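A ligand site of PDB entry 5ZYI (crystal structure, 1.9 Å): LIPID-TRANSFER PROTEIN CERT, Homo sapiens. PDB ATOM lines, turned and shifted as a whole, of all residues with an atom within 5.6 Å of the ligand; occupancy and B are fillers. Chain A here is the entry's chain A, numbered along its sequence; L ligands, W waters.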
ATOM      1  N   PHE A  75      18.649  15.968   7.310  1.00  0.00           N
ATOM      2  CA  PHE A  75      17.665  16.402   6.340  1.00  0.00           C
ATOM      3  C   PHE A  75      16.277  16.041   6.880  1.00  0.00           C
ATOM      4  O   PHE A  75      15.354  16.854   6.805  1.00  0.00           O
ATOM      5  CB  PHE A  75      18.005  15.859   4.950  1.00  0.00           C
ATOM      6  CG  PHE A  75      17.106  16.352   3.845  1.00  0.00           C
ATOM      7  CD1 PHE A  75      17.046  17.709   3.535  1.00  0.00           C
ATOM      8  CD2 PHE A  75      16.320  15.466   3.121  1.00  0.00           C
ATOM      9  CE1 PHE A  75      16.208  18.150   2.521  1.00  0.00           C
ATOM     10  CE2 PHE A  75      15.474  15.910   2.112  1.00  0.00           C
ATOM     11  CZ  PHE A  75      15.440  17.247   1.792  1.00  0.00           C
ATOM     12  N   ARG A  81      15.147  21.509  11.543  1.00  0.00           N
ATOM     13  CA  ARG A  81      14.671  22.156  10.332  1.00  0.00           C
ATOM     14  C   ARG A  81      14.935  23.665  10.389  1.00  0.00           C
ATOM     15  O   ARG A  81      15.514  24.214   9.461  1.00  0.00           O
ATOM     16  CB  ARG A  81      13.208  21.800  10.108  1.00  0.00           C
ATOM     17  CG  ARG A  81      12.649  22.264   8.770  1.00  0.00           C
ATOM     18  CD  ARG A  81      13.160  21.504   7.547  1.00  0.00           C
ATOM     19  NE  ARG A  81      13.310  20.053   7.716  1.00  0.00           N
ATOM     20  CZ  ARG A  81      12.343  19.157   7.509  1.00  0.00           C
ATOM     21  NH1 ARG A  81      12.591  17.870   7.654  1.00  0.00           N
ATOM     22  NH2 ARG A  81      11.116  19.556   7.192  1.00  0.00           N
ATOM     23  N   TRP A  84      18.332  25.307   9.286  1.00  0.00           N
ATOM     24  CA  TRP A  84      18.928  25.392   7.971  1.00  0.00           C
ATOM     25  C   TRP A  84      17.921  25.882   6.927  1.00  0.00           C
ATOM     26  O   TRP A  84      18.301  26.477   5.925  1.00  0.00           O
ATOM     27  CB  TRP A  84      19.662  24.089   7.584  1.00  0.00           C
ATOM     28  CG  TRP A  84      18.767  22.895   7.591  1.00  0.00           C
ATOM     29  CD1 TRP A  84      18.679  21.943   8.572  1.00  0.00           C
ATOM     30  CD2 TRP A  84      17.859  22.488   6.548  1.00  0.00           C
ATOM     31  NE1 TRP A  84      17.746  20.993   8.236  1.00  0.00           N
ATOM     32  CE2 TRP A  84      17.245  21.286   6.991  1.00  0.00           C
ATOM     33  CE3 TRP A  84      17.521  22.994   5.284  1.00  0.00           C
ATOM     34  CZ2 TRP A  84      16.284  20.628   6.217  1.00  0.00           C
ATOM     35  CZ3 TRP A  84      16.551  22.367   4.540  1.00  0.00           C
ATOM     36  CH2 TRP A  84      15.953  21.189   4.997  1.00  0.00           C
ATOM     37  N   GLU A  85      16.619  25.684   7.190  1.00  0.00           N
ATOM     38  CA  GLU A  85      15.555  26.083   6.277  1.00  0.00           C
ATOM     39  C   GLU A  85      15.478  27.601   6.228  1.00  0.00           C
ATOM     40  O   GLU A  85      15.482  28.229   7.295  1.00  0.00           O
ATOM     41  CB  GLU A  85      14.208  25.599   6.815  1.00  0.00           C
ATOM     42  CG  GLU A  85      13.894  24.141   6.538  1.00  0.00           C
ATOM     43  CD  GLU A  85      13.236  23.883   5.191  1.00  0.00           C
ATOM     44  OE1 GLU A  85      12.282  23.122   5.155  1.00  0.00           O
ATOM     45  OE2 GLU A  85      13.695  24.460   4.185  1.00  0.00           O
ATOM     46  N   THR A  87      13.112  29.160   3.701  1.00  0.00           N
ATOM     47  CA  THR A  87      11.968  29.508   2.872  1.00  0.00           C
ATOM     48  C   THR A  87      10.646  29.092   3.511  1.00  0.00           C
ATOM     49  O   THR A  87       9.598  29.265   2.886  1.00  0.00           O
ATOM     50  CB  THR A  87      12.057  28.913   1.458  1.00  0.00           C
ATOM     51  OG1 THR A  87      11.947  27.488   1.506  1.00  0.00           O
ATOM     52  CG2 THR A  87      13.307  29.295   0.688  1.00  0.00           C
ATOM     53  N   ILE A  88      10.688  28.574   4.743  1.00  0.00           N
ATOM     54  CA  ILE A  88       9.516  28.045   5.445  1.00  0.00           C
ATOM     55  C   ILE A  88       9.018  29.135   6.405  1.00  0.00           C
ATOM     56  O   ILE A  88       9.793  29.654   7.192  1.00  0.00           O
ATOM     57  CB  ILE A  88       9.949  26.814   6.278  1.00  0.00           C
ATOM     58  CG1 ILE A  88      10.460  25.657   5.418  1.00  0.00           C
ATOM     59  CG2 ILE A  88       8.840  26.346   7.214  1.00  0.00           C
ATOM     60  CD1 ILE A  88       9.421  25.099   4.509  1.00  0.00           C
ATOM     61  N   GLN A 106       3.417  22.336   5.743  1.00  0.00           N
ATOM     62  CA  GLN A 106       4.300  23.489   5.860  1.00  0.00           C
ATOM     63  C   GLN A 106       3.879  24.561   4.867  1.00  0.00           C
ATOM     64  O   GLN A 106       3.293  24.237   3.832  1.00  0.00           O
ATOM     65  CB  GLN A 106       5.780  23.154   5.690  1.00  0.00           C
ATOM     66  CG  GLN A 106       6.222  22.866   4.248  1.00  0.00           C
ATOM     67  CD  GLN A 106       7.612  22.253   4.174  1.00  0.00           C
ATOM     68  OE1 GLN A 106       8.152  21.723   5.164  1.00  0.00           O
ATOM     69  NE2 GLN A 106       8.244  22.382   3.005  1.00  0.00           N
ATOM     70  N   HIS A 108       5.340  28.053   2.801  1.00  0.00           N
ATOM     71  CA  HIS A 108       6.528  28.720   2.308  1.00  0.00           C
ATOM     72  C   HIS A 108       6.328  30.226   2.337  1.00  0.00           C
ATOM     73  O   HIS A 108       5.223  30.694   2.101  1.00  0.00           O
ATOM     74  CB  HIS A 108       6.858  28.150   0.912  1.00  0.00           C
ATOM     75  CG  HIS A 108       7.415  26.771   1.036  1.00  0.00           C
ATOM     76  ND1 HIS A 108       8.777  26.543   1.163  1.00  0.00           N
ATOM     77  CD2 HIS A 108       6.799  25.569   1.150  1.00  0.00           C
ATOM     78  CE1 HIS A 108       8.989  25.232   1.281  1.00  0.00           C
ATOM     79  NE2 HIS A 108       7.789  24.627   1.316  1.00  0.00           N
ATOM     80  N   VAL A 111       6.616  34.491  -2.449  1.00  0.00           N
ATOM     81  CA  VAL A 111       7.531  35.253  -3.286  1.00  0.00           C
ATOM     82  C   VAL A 111       6.719  36.176  -4.201  1.00  0.00           C
ATOM     83  O   VAL A 111       6.024  35.735  -5.100  1.00  0.00           O
ATOM     84  CB  VAL A 111       8.519  34.382  -4.094  1.00  0.00           C
ATOM     85  CG1 VAL A 111       7.817  33.446  -5.059  1.00  0.00           C
ATOM     86  CG2 VAL A 111       9.533  35.252  -4.845  1.00  0.00           C
ATOM     87  N   ALA A 114       3.549  36.008  -6.626  1.00  0.00           N
ATOM     88  CA  ALA A 114       2.723  34.823  -6.630  1.00  0.00           C
ATOM     89  C   ALA A 114       2.057  34.656  -5.260  1.00  0.00           C
ATOM     90  O   ALA A 114       2.510  35.202  -4.265  1.00  0.00           O
ATOM     91  CB  ALA A 114       3.558  33.607  -6.991  1.00  0.00           C
ATOM     92  N   SER A 115       0.948  33.938  -5.214  1.00  0.00           N
ATOM     93  CA  SER A 115       0.386  33.718  -3.890  1.00  0.00           C
ATOM     94  C   SER A 115       1.216  32.680  -3.143  1.00  0.00           C
ATOM     95  O   SER A 115       2.019  31.952  -3.712  1.00  0.00           O
ATOM     96  CB  SER A 115      -1.078  33.395  -3.892  1.00  0.00           C
ATOM     97  OG  SER A 115      -1.424  32.524  -4.937  1.00  0.00           O
ATOM     98  N   ARG A 117       2.280  29.379  -1.189  1.00  0.00           N
ATOM     99  CA  ARG A 117       2.091  27.932  -1.375  1.00  0.00           C
ATOM    100  C   ARG A 117       2.202  27.224  -0.027  1.00  0.00           C
ATOM    101  O   ARG A 117       3.030  27.595   0.802  1.00  0.00           O
ATOM    102  CB  ARG A 117       3.142  27.347  -2.321  1.00  0.00           C
ATOM    103  CG  ARG A 117       2.622  27.172  -3.750  1.00  0.00           C
ATOM    104  CD  ARG A 117       2.338  28.522  -4.424  1.00  0.00           C
ATOM    105  NE  ARG A 117       1.806  28.352  -5.746  1.00  0.00           N
ATOM    106  CZ  ARG A 117       1.210  29.287  -6.474  1.00  0.00           C
ATOM    107  NH1 ARG A 117       1.057  30.527  -6.006  1.00  0.00           N
ATOM    108  NH2 ARG A 117       0.776  28.969  -7.669  1.00  0.00           N
ATOM    109  N   VAL A 119       2.227  22.890   1.446  1.00  0.00           N
ATOM    110  CA  VAL A 119       2.502  21.527   1.040  1.00  0.00           C
ATOM    111  C   VAL A 119       2.101  20.576   2.177  1.00  0.00           C
ATOM    112  O   VAL A 119       2.213  20.922   3.360  1.00  0.00           O
ATOM    113  CB  VAL A 119       3.995  21.339   0.764  1.00  0.00           C
ATOM    114  CG1 VAL A 119       4.235  20.077  -0.094  1.00  0.00           C
ATOM    115  CG2 VAL A 119       4.572  22.571   0.073  1.00  0.00           C
ATOM    116  N   TYR A 121       2.992  16.517   3.008  1.00  0.00           N
ATOM    117  CA  TYR A 121       3.792  15.471   2.407  1.00  0.00           C
ATOM    118  C   TYR A 121       4.243  14.490   3.482  1.00  0.00           C
ATOM    119  O   TYR A 121       4.512  14.893   4.622  1.00  0.00           O
ATOM    120  CB  TYR A 121       5.015  16.092   1.690  1.00  0.00           C
ATOM    121  CG  TYR A 121       5.986  16.832   2.578  1.00  0.00           C
ATOM    122  CD1 TYR A 121       5.808  18.186   2.839  1.00  0.00           C
ATOM    123  CD2 TYR A 121       7.123  16.214   3.078  1.00  0.00           C
ATOM    124  CE1 TYR A 121       6.722  18.878   3.641  1.00  0.00           C
ATOM    125  CE2 TYR A 121       8.068  16.902   3.837  1.00  0.00           C
ATOM    126  CZ  TYR A 121       7.847  18.245   4.129  1.00  0.00           C
ATOM    127  OH  TYR A 121       8.766  18.944   4.883  1.00  0.00           O
ATOM    128  N   ASN A 143      10.494  12.823   0.340  1.00  0.00           N
ATOM    129  CA  ASN A 143       9.381  13.685   0.713  1.00  0.00           C
ATOM    130  C   ASN A 143       8.398  13.723  -0.458  1.00  0.00           C
ATOM    131  O   ASN A 143       8.712  14.272  -1.540  1.00  0.00           O
ATOM    132  CB  ASN A 143       9.902  15.106   1.052  1.00  0.00           C
ATOM    133  CG  ASN A 143      10.857  15.132   2.230  1.00  0.00           C
ATOM    134  OD1 ASN A 143      10.748  14.300   3.137  1.00  0.00           O
ATOM    135  ND2 ASN A 143      11.784  16.088   2.265  1.00  0.00           N
ATOM    136  N   ALA A 160       0.797  23.106  -3.209  1.00  0.00           N
ATOM    137  CA  ALA A 160       1.784  22.556  -4.153  1.00  0.00           C
ATOM    138  C   ALA A 160       1.900  21.053  -3.924  1.00  0.00           C
ATOM    139  O   ALA A 160       1.567  20.595  -2.831  1.00  0.00           O
ATOM    140  CB  ALA A 160       3.125  23.208  -3.870  1.00  0.00           C
ATOM    141  N   ILE A 162       4.738  17.797  -4.262  1.00  0.00           N
ATOM    142  CA  ILE A 162       6.179  17.593  -4.356  1.00  0.00           C
ATOM    143  C   ILE A 162       6.476  16.102  -4.373  1.00  0.00           C
ATOM    144  O   ILE A 162       5.698  15.278  -3.874  1.00  0.00           O
ATOM    145  CB  ILE A 162       6.965  18.316  -3.245  1.00  0.00           C
ATOM    146  CG1 ILE A 162       6.830  17.611  -1.878  1.00  0.00           C
ATOM    147  CG2 ILE A 162       6.565  19.785  -3.189  1.00  0.00           C
ATOM    148  CD1 ILE A 162       7.767  18.154  -0.806  1.00  0.00           C
ATOM    149  N   VAL A 164      10.357  14.638  -3.722  1.00  0.00           N
ATOM    150  CA  VAL A 164      11.699  15.121  -3.521  1.00  0.00           C
ATOM    151  C   VAL A 164      12.457  13.930  -2.969  1.00  0.00           C
ATOM    152  O   VAL A 164      11.879  13.161  -2.195  1.00  0.00           O
ATOM    153  CB  VAL A 164      11.703  16.338  -2.578  1.00  0.00           C
ATOM    154  CG1 VAL A 164      13.058  16.559  -1.954  1.00  0.00           C
ATOM    155  CG2 VAL A 164      11.132  17.624  -3.198  1.00  0.00           C
ATOM    156  N   TYR A 192      20.257  14.924  -5.383  1.00  0.00           N
ATOM    157  CA  TYR A 192      19.057  15.561  -4.857  1.00  0.00           C
ATOM    158  C   TYR A 192      18.110  15.772  -6.038  1.00  0.00           C
ATOM    159  O   TYR A 192      18.497  16.378  -7.052  1.00  0.00           O
ATOM    160  CB  TYR A 192      19.430  16.869  -4.149  1.00  0.00           C
ATOM    161  CG  TYR A 192      18.222  17.703  -3.780  1.00  0.00           C
ATOM    162  CD1 TYR A 192      17.558  17.452  -2.595  1.00  0.00           C
ATOM    163  CD2 TYR A 192      17.699  18.678  -4.632  1.00  0.00           C
ATOM    164  CE1 TYR A 192      16.411  18.167  -2.237  1.00  0.00           C
ATOM    165  CE2 TYR A 192      16.551  19.390  -4.313  1.00  0.00           C
ATOM    166  CZ  TYR A 192      15.936  19.165  -3.083  1.00  0.00           C
ATOM    167  OH  TYR A 192      14.808  19.831  -2.733  1.00  0.00           O
ATOM    168  N   VAL A 196       8.370  19.522  -8.411  1.00  0.00           N
ATOM    169  CA  VAL A 196       7.389  20.317  -7.675  1.00  0.00           C
ATOM    170  C   VAL A 196       6.336  20.789  -8.651  1.00  0.00           C
ATOM    171  O   VAL A 196       6.678  21.392  -9.677  1.00  0.00           O
ATOM    172  CB  VAL A 196       8.065  21.509  -6.969  1.00  0.00           C
ATOM    173  CG1 VAL A 196       7.072  22.485  -6.298  1.00  0.00           C
ATOM    174  CG2 VAL A 196       9.154  21.073  -6.024  1.00  0.00           C
ATOM    175  N   PRO A 198       3.615  23.567  -8.603  1.00  0.00           N
ATOM    176  CA  PRO A 198       3.238  24.654  -7.702  1.00  0.00           C
ATOM    177  C   PRO A 198       1.732  24.922  -7.582  1.00  0.00           C
ATOM    178  O   PRO A 198       1.295  25.693  -6.727  1.00  0.00           O
ATOM    179  CB  PRO A 198       3.974  25.900  -8.271  1.00  0.00           C
ATOM    180  CG  PRO A 198       4.228  25.545  -9.730  1.00  0.00           C
ATOM    181  CD  PRO A 198       4.328  24.021  -9.808  1.00  0.00           C
ATOM    182  N   ALA A 202       1.365  30.581 -11.496  1.00  0.00           N
ATOM    183  CA  ALA A 202       2.299  31.558 -10.967  1.00  0.00           C
ATOM    184  C   ALA A 202       3.067  31.983 -12.190  1.00  0.00           C
ATOM    185  O   ALA A 202       3.092  31.203 -13.141  1.00  0.00           O
ATOM    186  CB  ALA A 202       3.201  30.917  -9.950  1.00  0.00           C
ATOM    187  N   VAL A 206       8.819  34.019 -12.440  1.00  0.00           N
ATOM    188  CA  VAL A 206       8.949  33.993 -11.004  1.00  0.00           C
ATOM    189  C   VAL A 206       9.391  32.594 -10.552  1.00  0.00           C
ATOM    190  O   VAL A 206      10.360  32.440  -9.813  1.00  0.00           O
ATOM    191  CB  VAL A 206       7.630  34.432 -10.344  1.00  0.00           C
ATOM    192  CG1 VAL A 206       7.701  34.304  -8.831  1.00  0.00           C
ATOM    193  CG2 VAL A 206       7.258  35.858 -10.740  1.00  0.00           C
ATOM    194  N   LEU A 207       8.709  31.555 -11.031  1.00  0.00           N
ATOM    195  CA  LEU A 207       9.027  30.191 -10.628  1.00  0.00           C
ATOM    196  C   LEU A 207      10.465  29.867 -10.991  1.00  0.00           C
ATOM    197  O   LEU A 207      11.171  29.337 -10.158  1.00  0.00           O
ATOM    198  CB  LEU A 207       8.042  29.216 -11.287  1.00  0.00           C
ATOM    199  CG  LEU A 207       6.634  29.328 -10.675  1.00  0.00           C
ATOM    200  CD1 LEU A 207       5.601  28.605 -11.532  1.00  0.00           C
ATOM    201  CD2 LEU A 207       6.611  28.807  -9.247  1.00  0.00           C
ATOM    202  N   VAL A 210      12.932  31.742  -8.752  1.00  0.00           N
ATOM    203  CA  VAL A 210      12.961  31.257  -7.387  1.00  0.00           C
ATOM    204  C   VAL A 210      13.747  29.943  -7.368  1.00  0.00           C
ATOM    205  O   VAL A 210      14.605  29.752  -6.507  1.00  0.00           O
ATOM    206  CB  VAL A 210      11.556  31.109  -6.786  1.00  0.00           C
ATOM    207  CG1 VAL A 210      11.623  30.373  -5.437  1.00  0.00           C
ATOM    208  CG2 VAL A 210      10.842  32.446  -6.617  1.00  0.00           C
ATOM    209  N   ALA A 211      13.543  29.062  -8.364  1.00  0.00           N
ATOM    210  CA  ALA A 211      14.252  27.788  -8.345  1.00  0.00           C
ATOM    211  C   ALA A 211      15.753  28.017  -8.489  1.00  0.00           C
ATOM    212  O   ALA A 211      16.594  27.384  -7.838  1.00  0.00           O
ATOM    213  CB  ALA A 211      13.727  26.883  -9.424  1.00  0.00           C
ATOM    214  N   GLU A 214      17.064  29.533  -5.169  1.00  0.00           N
ATOM    215  CA  GLU A 214      16.848  28.866  -3.899  1.00  0.00           C
ATOM    216  C   GLU A 214      17.495  27.473  -3.819  1.00  0.00           C
ATOM    217  O   GLU A 214      17.958  27.097  -2.746  1.00  0.00           O
ATOM    218  CB  GLU A 214      15.356  28.882  -3.522  1.00  0.00           C
ATOM    219  CG  GLU A 214      14.806  30.265  -3.183  1.00  0.00           C
ATOM    220  CD  GLU A 214      15.542  31.071  -2.120  1.00  0.00           C
ATOM    221  OE1 GLU A 214      16.128  30.442  -1.210  1.00  0.00           O
ATOM    222  OE2 GLU A 214      15.540  32.340  -2.205  1.00  0.00           O
ATOM    223  N   TYR A 215      17.522  26.686  -4.910  1.00  0.00           N
ATOM    224  CA  TYR A 215      18.096  25.330  -4.822  1.00  0.00           C
ATOM    225  C   TYR A 215      19.594  25.364  -4.519  1.00  0.00           C
ATOM    226  O   TYR A 215      20.054  24.669  -3.588  1.00  0.00           O
ATOM    227  CB  TYR A 215      17.721  24.432  -6.009  1.00  0.00           C
ATOM    228  CG  TYR A 215      16.282  23.946  -6.007  1.00  0.00           C
ATOM    229  CD1 TYR A 215      15.781  23.095  -5.017  1.00  0.00           C
ATOM    230  CD2 TYR A 215      15.411  24.333  -7.013  1.00  0.00           C
ATOM    231  CE1 TYR A 215      14.463  22.623  -5.042  1.00  0.00           C
ATOM    232  CE2 TYR A 215      14.108  23.870  -7.055  1.00  0.00           C
ATOM    233  CZ  TYR A 215      13.624  22.994  -6.085  1.00  0.00           C
ATOM    234  OH  TYR A 215      12.306  22.588  -6.169  1.00  0.00           O
ATOM    235  N   PHE A 218      20.130  26.475  -0.956  1.00  0.00           N
ATOM    236  CA  PHE A 218      19.693  25.427  -0.036  1.00  0.00           C
ATOM    237  C   PHE A 218      20.799  24.385   0.084  1.00  0.00           C
ATOM    238  O   PHE A 218      21.241  24.099   1.183  1.00  0.00           O
ATOM    239  CB  PHE A 218      18.339  24.835  -0.433  1.00  0.00           C
ATOM    240  CG  PHE A 218      18.223  23.360  -0.120  1.00  0.00           C
ATOM    241  CD1 PHE A 218      18.069  22.934   1.190  1.00  0.00           C
ATOM    242  CD2 PHE A 218      18.312  22.400  -1.110  1.00  0.00           C
ATOM    243  CE1 PHE A 218      17.951  21.586   1.471  1.00  0.00           C
ATOM    244  CE2 PHE A 218      18.224  21.030  -0.830  1.00  0.00           C
ATOM    245  CZ  PHE A 218      18.052  20.633   0.478  1.00  0.00           C
HETATM  246  C1  LIG L   1      10.162  20.876  -0.308  1.00  0.00           C
HETATM  247  C2  LIG L   1       9.727  25.937  -5.647  1.00  0.00           C
HETATM  248  C3  LIG L   1      11.187  26.420  -5.564  1.00  0.00           C
HETATM  249  C4  LIG L   1      13.246  26.447  -1.870  1.00  0.00           C
HETATM  250  C5  LIG L   1      13.211  25.774  -4.202  1.00  0.00           C
HETATM  251  C6  LIG L   1      11.967  26.409  -4.301  1.00  0.00           C
HETATM  252  C7  LIG L   1      11.989  27.055  -2.034  1.00  0.00           C
HETATM  253  C8  LIG L   1      12.940  20.331   2.182  1.00  0.00           C
HETATM  254  N1  LIG L   1      11.355  27.054  -3.239  1.00  0.00           N
HETATM  255  C9  LIG L   1       9.807  24.381  -3.690  1.00  0.00           C
HETATM  256  C10 LIG L   1       9.200  23.686  -2.623  1.00  0.00           C
HETATM  257  C11 LIG L   1      11.542  20.950  -0.374  1.00  0.00           C
HETATM  258  C12 LIG L   1      11.425  22.746  -1.928  1.00  0.00           C
HETATM  259  O1  LIG L   1      13.805  19.583  -0.123  1.00  0.00           O
HETATM  260  S1  LIG L   1      12.475  19.712   0.525  1.00  0.00           S
HETATM  261  O2  LIG L   1      11.523  18.599   0.673  1.00  0.00           O
HETATM  262  C13 LIG L   1      11.746  20.476   3.151  1.00  0.00           C
HETATM  263  O3  LIG L   1      11.096  21.691   2.877  1.00  0.00           O
HETATM  264  C14 LIG L   1      12.243  21.872  -1.168  1.00  0.00           C
HETATM  265  C15 LIG L   1      10.016  22.735  -1.856  1.00  0.00           C
HETATM  266  C16 LIG L   1       9.367  21.779  -1.045  1.00  0.00           C
HETATM  267  C17 LIG L   1       9.058  25.263  -4.461  1.00  0.00           C
HETATM  268  C18 LIG L   1       7.702  25.508  -4.130  1.00  0.00           C
HETATM  269  C19 LIG L   1       6.897  26.458  -5.026  1.00  0.00           C
HETATM  270  C20 LIG L   1       6.784  27.845  -4.336  1.00  0.00           C
HETATM  271  C21 LIG L   1       6.006  28.689  -5.353  1.00  0.00           C
HETATM  272  C22 LIG L   1       6.502  30.119  -5.290  1.00  0.00           C
HETATM  273  C23 LIG L   1       5.620  30.999  -6.183  1.00  0.00           C
HETATM  274  C24 LIG L   1       7.065  24.807  -3.086  1.00  0.00           C
HETATM  275  C25 LIG L   1       7.837  23.904  -2.311  1.00  0.00           C
HETATM  276  C26 LIG L   1      10.037  27.393  -5.577  1.00  0.00           C
HETATM  277  C27 LIG L   1      13.896  25.817  -2.972  1.00  0.00           C
HETATM  278  O   HOH W   1      12.404  23.786   1.914  1.00  0.00           O
HETATM  279  O   HOH W   2       4.831  32.676  -3.487  1.00  0.00           O
HETATM  280  O   HOH W   3       9.503  25.135  -8.954  1.00  0.00           O
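An oxygen (O2) of the ligand lies within hydrogen-bond range of the side-chain amide nitrogen of Asn 143, at 3.0 Å.
An oxygen (O3) of the ligand lies within hydrogen-bond range of the side-chain carboxylate (OE1) of Glu 85 (2.9 Å).
The side-chain amide nitrogen of Gln 106 lies within hydrogen-bond range of an oxygen (O3) of the ligand.
The side-chain hydroxyl (OH) of Tyr 192 is in hydrogen-bond range of an oxygen (O1) of the ligand (2.8 Å).
The guanidinium group (NE) of Arg 117 is in hydrogen-bond range of the backbone carbonyl oxygen (O) of Pro 198.
The backbone carbonyl oxygen (O) of Gln 106 is in hydrogen-bond range of the backbone NH (N) of Val 119 (2.9 Å).
The backbone NH (N) of His 108 sits at hydrogen-bond distance from the backbone carbonyl oxygen (O) of Arg 117 (3.1 Å).
A ring nitrogen (NE2) of His 108 lies within hydrogen-bond range of the side-chain amide nitrogen (NE2) of Gln 106, at 2.8 Å.
The backbone carbonyl oxygen of Phe 75 is in hydrogen-bond range of the guanidinium group of Arg 81, at 3.1 Å.
The backbone NH (N) of Val 164 is in hydrogen-bond range of the backbone carbonyl oxygen (O) of Asn 143, at 2.8 Å.
The backbone carbonyl oxygen of Thr 87 sits close to a ring nitrogen (ND1) of His 108 (3.3 Å).
The backbone carbonyl oxygen (O) of Ser 115 sits at hydrogen-bond distance from the guanidinium group (NH1) of Arg 117.
Phe 75 touches the ligand.
Thr 87 touches the ligand.
NE2 of His 108 touches C25 of the ligand, at 3.7 Å.
Val 111 touches the ligand.
Ala 114 touches the ligand (CB to C23, 3.4 Å).
CD of Arg 117 touches C21 of the ligand, 3.8 Å away.
Tyr 121 touches the ligand.
Ile 162 touches the ligand.
CG1 of Val 164 touches O1 of the ligand (3.6 Å).
CG1 of Val 196 touches C18 of the ligand (3.8 Å).
CD2 of Leu 207 touches C23 of the ligand, at 3.9 Å.
CG1 of Val 210 touches C26 of the ligand, 3.4 Å away.
CB of Glu 214 touches C27 of the ligand, 3.4 Å away.
CZ of Tyr 215 touches C5 of the ligand, at 3.4 Å.
Of the 29 residues printed, 18 come within 4 Å of the ligand.
Along chain A the residues within 4 Å of the ligand span positions 75 to 215.
Water W1 lies within hydrogen-bond range of an oxygen (O3) of the ligand (2.7 Å) and the side-chain carboxylate (OE2) of Glu 85 (2.7 Å).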
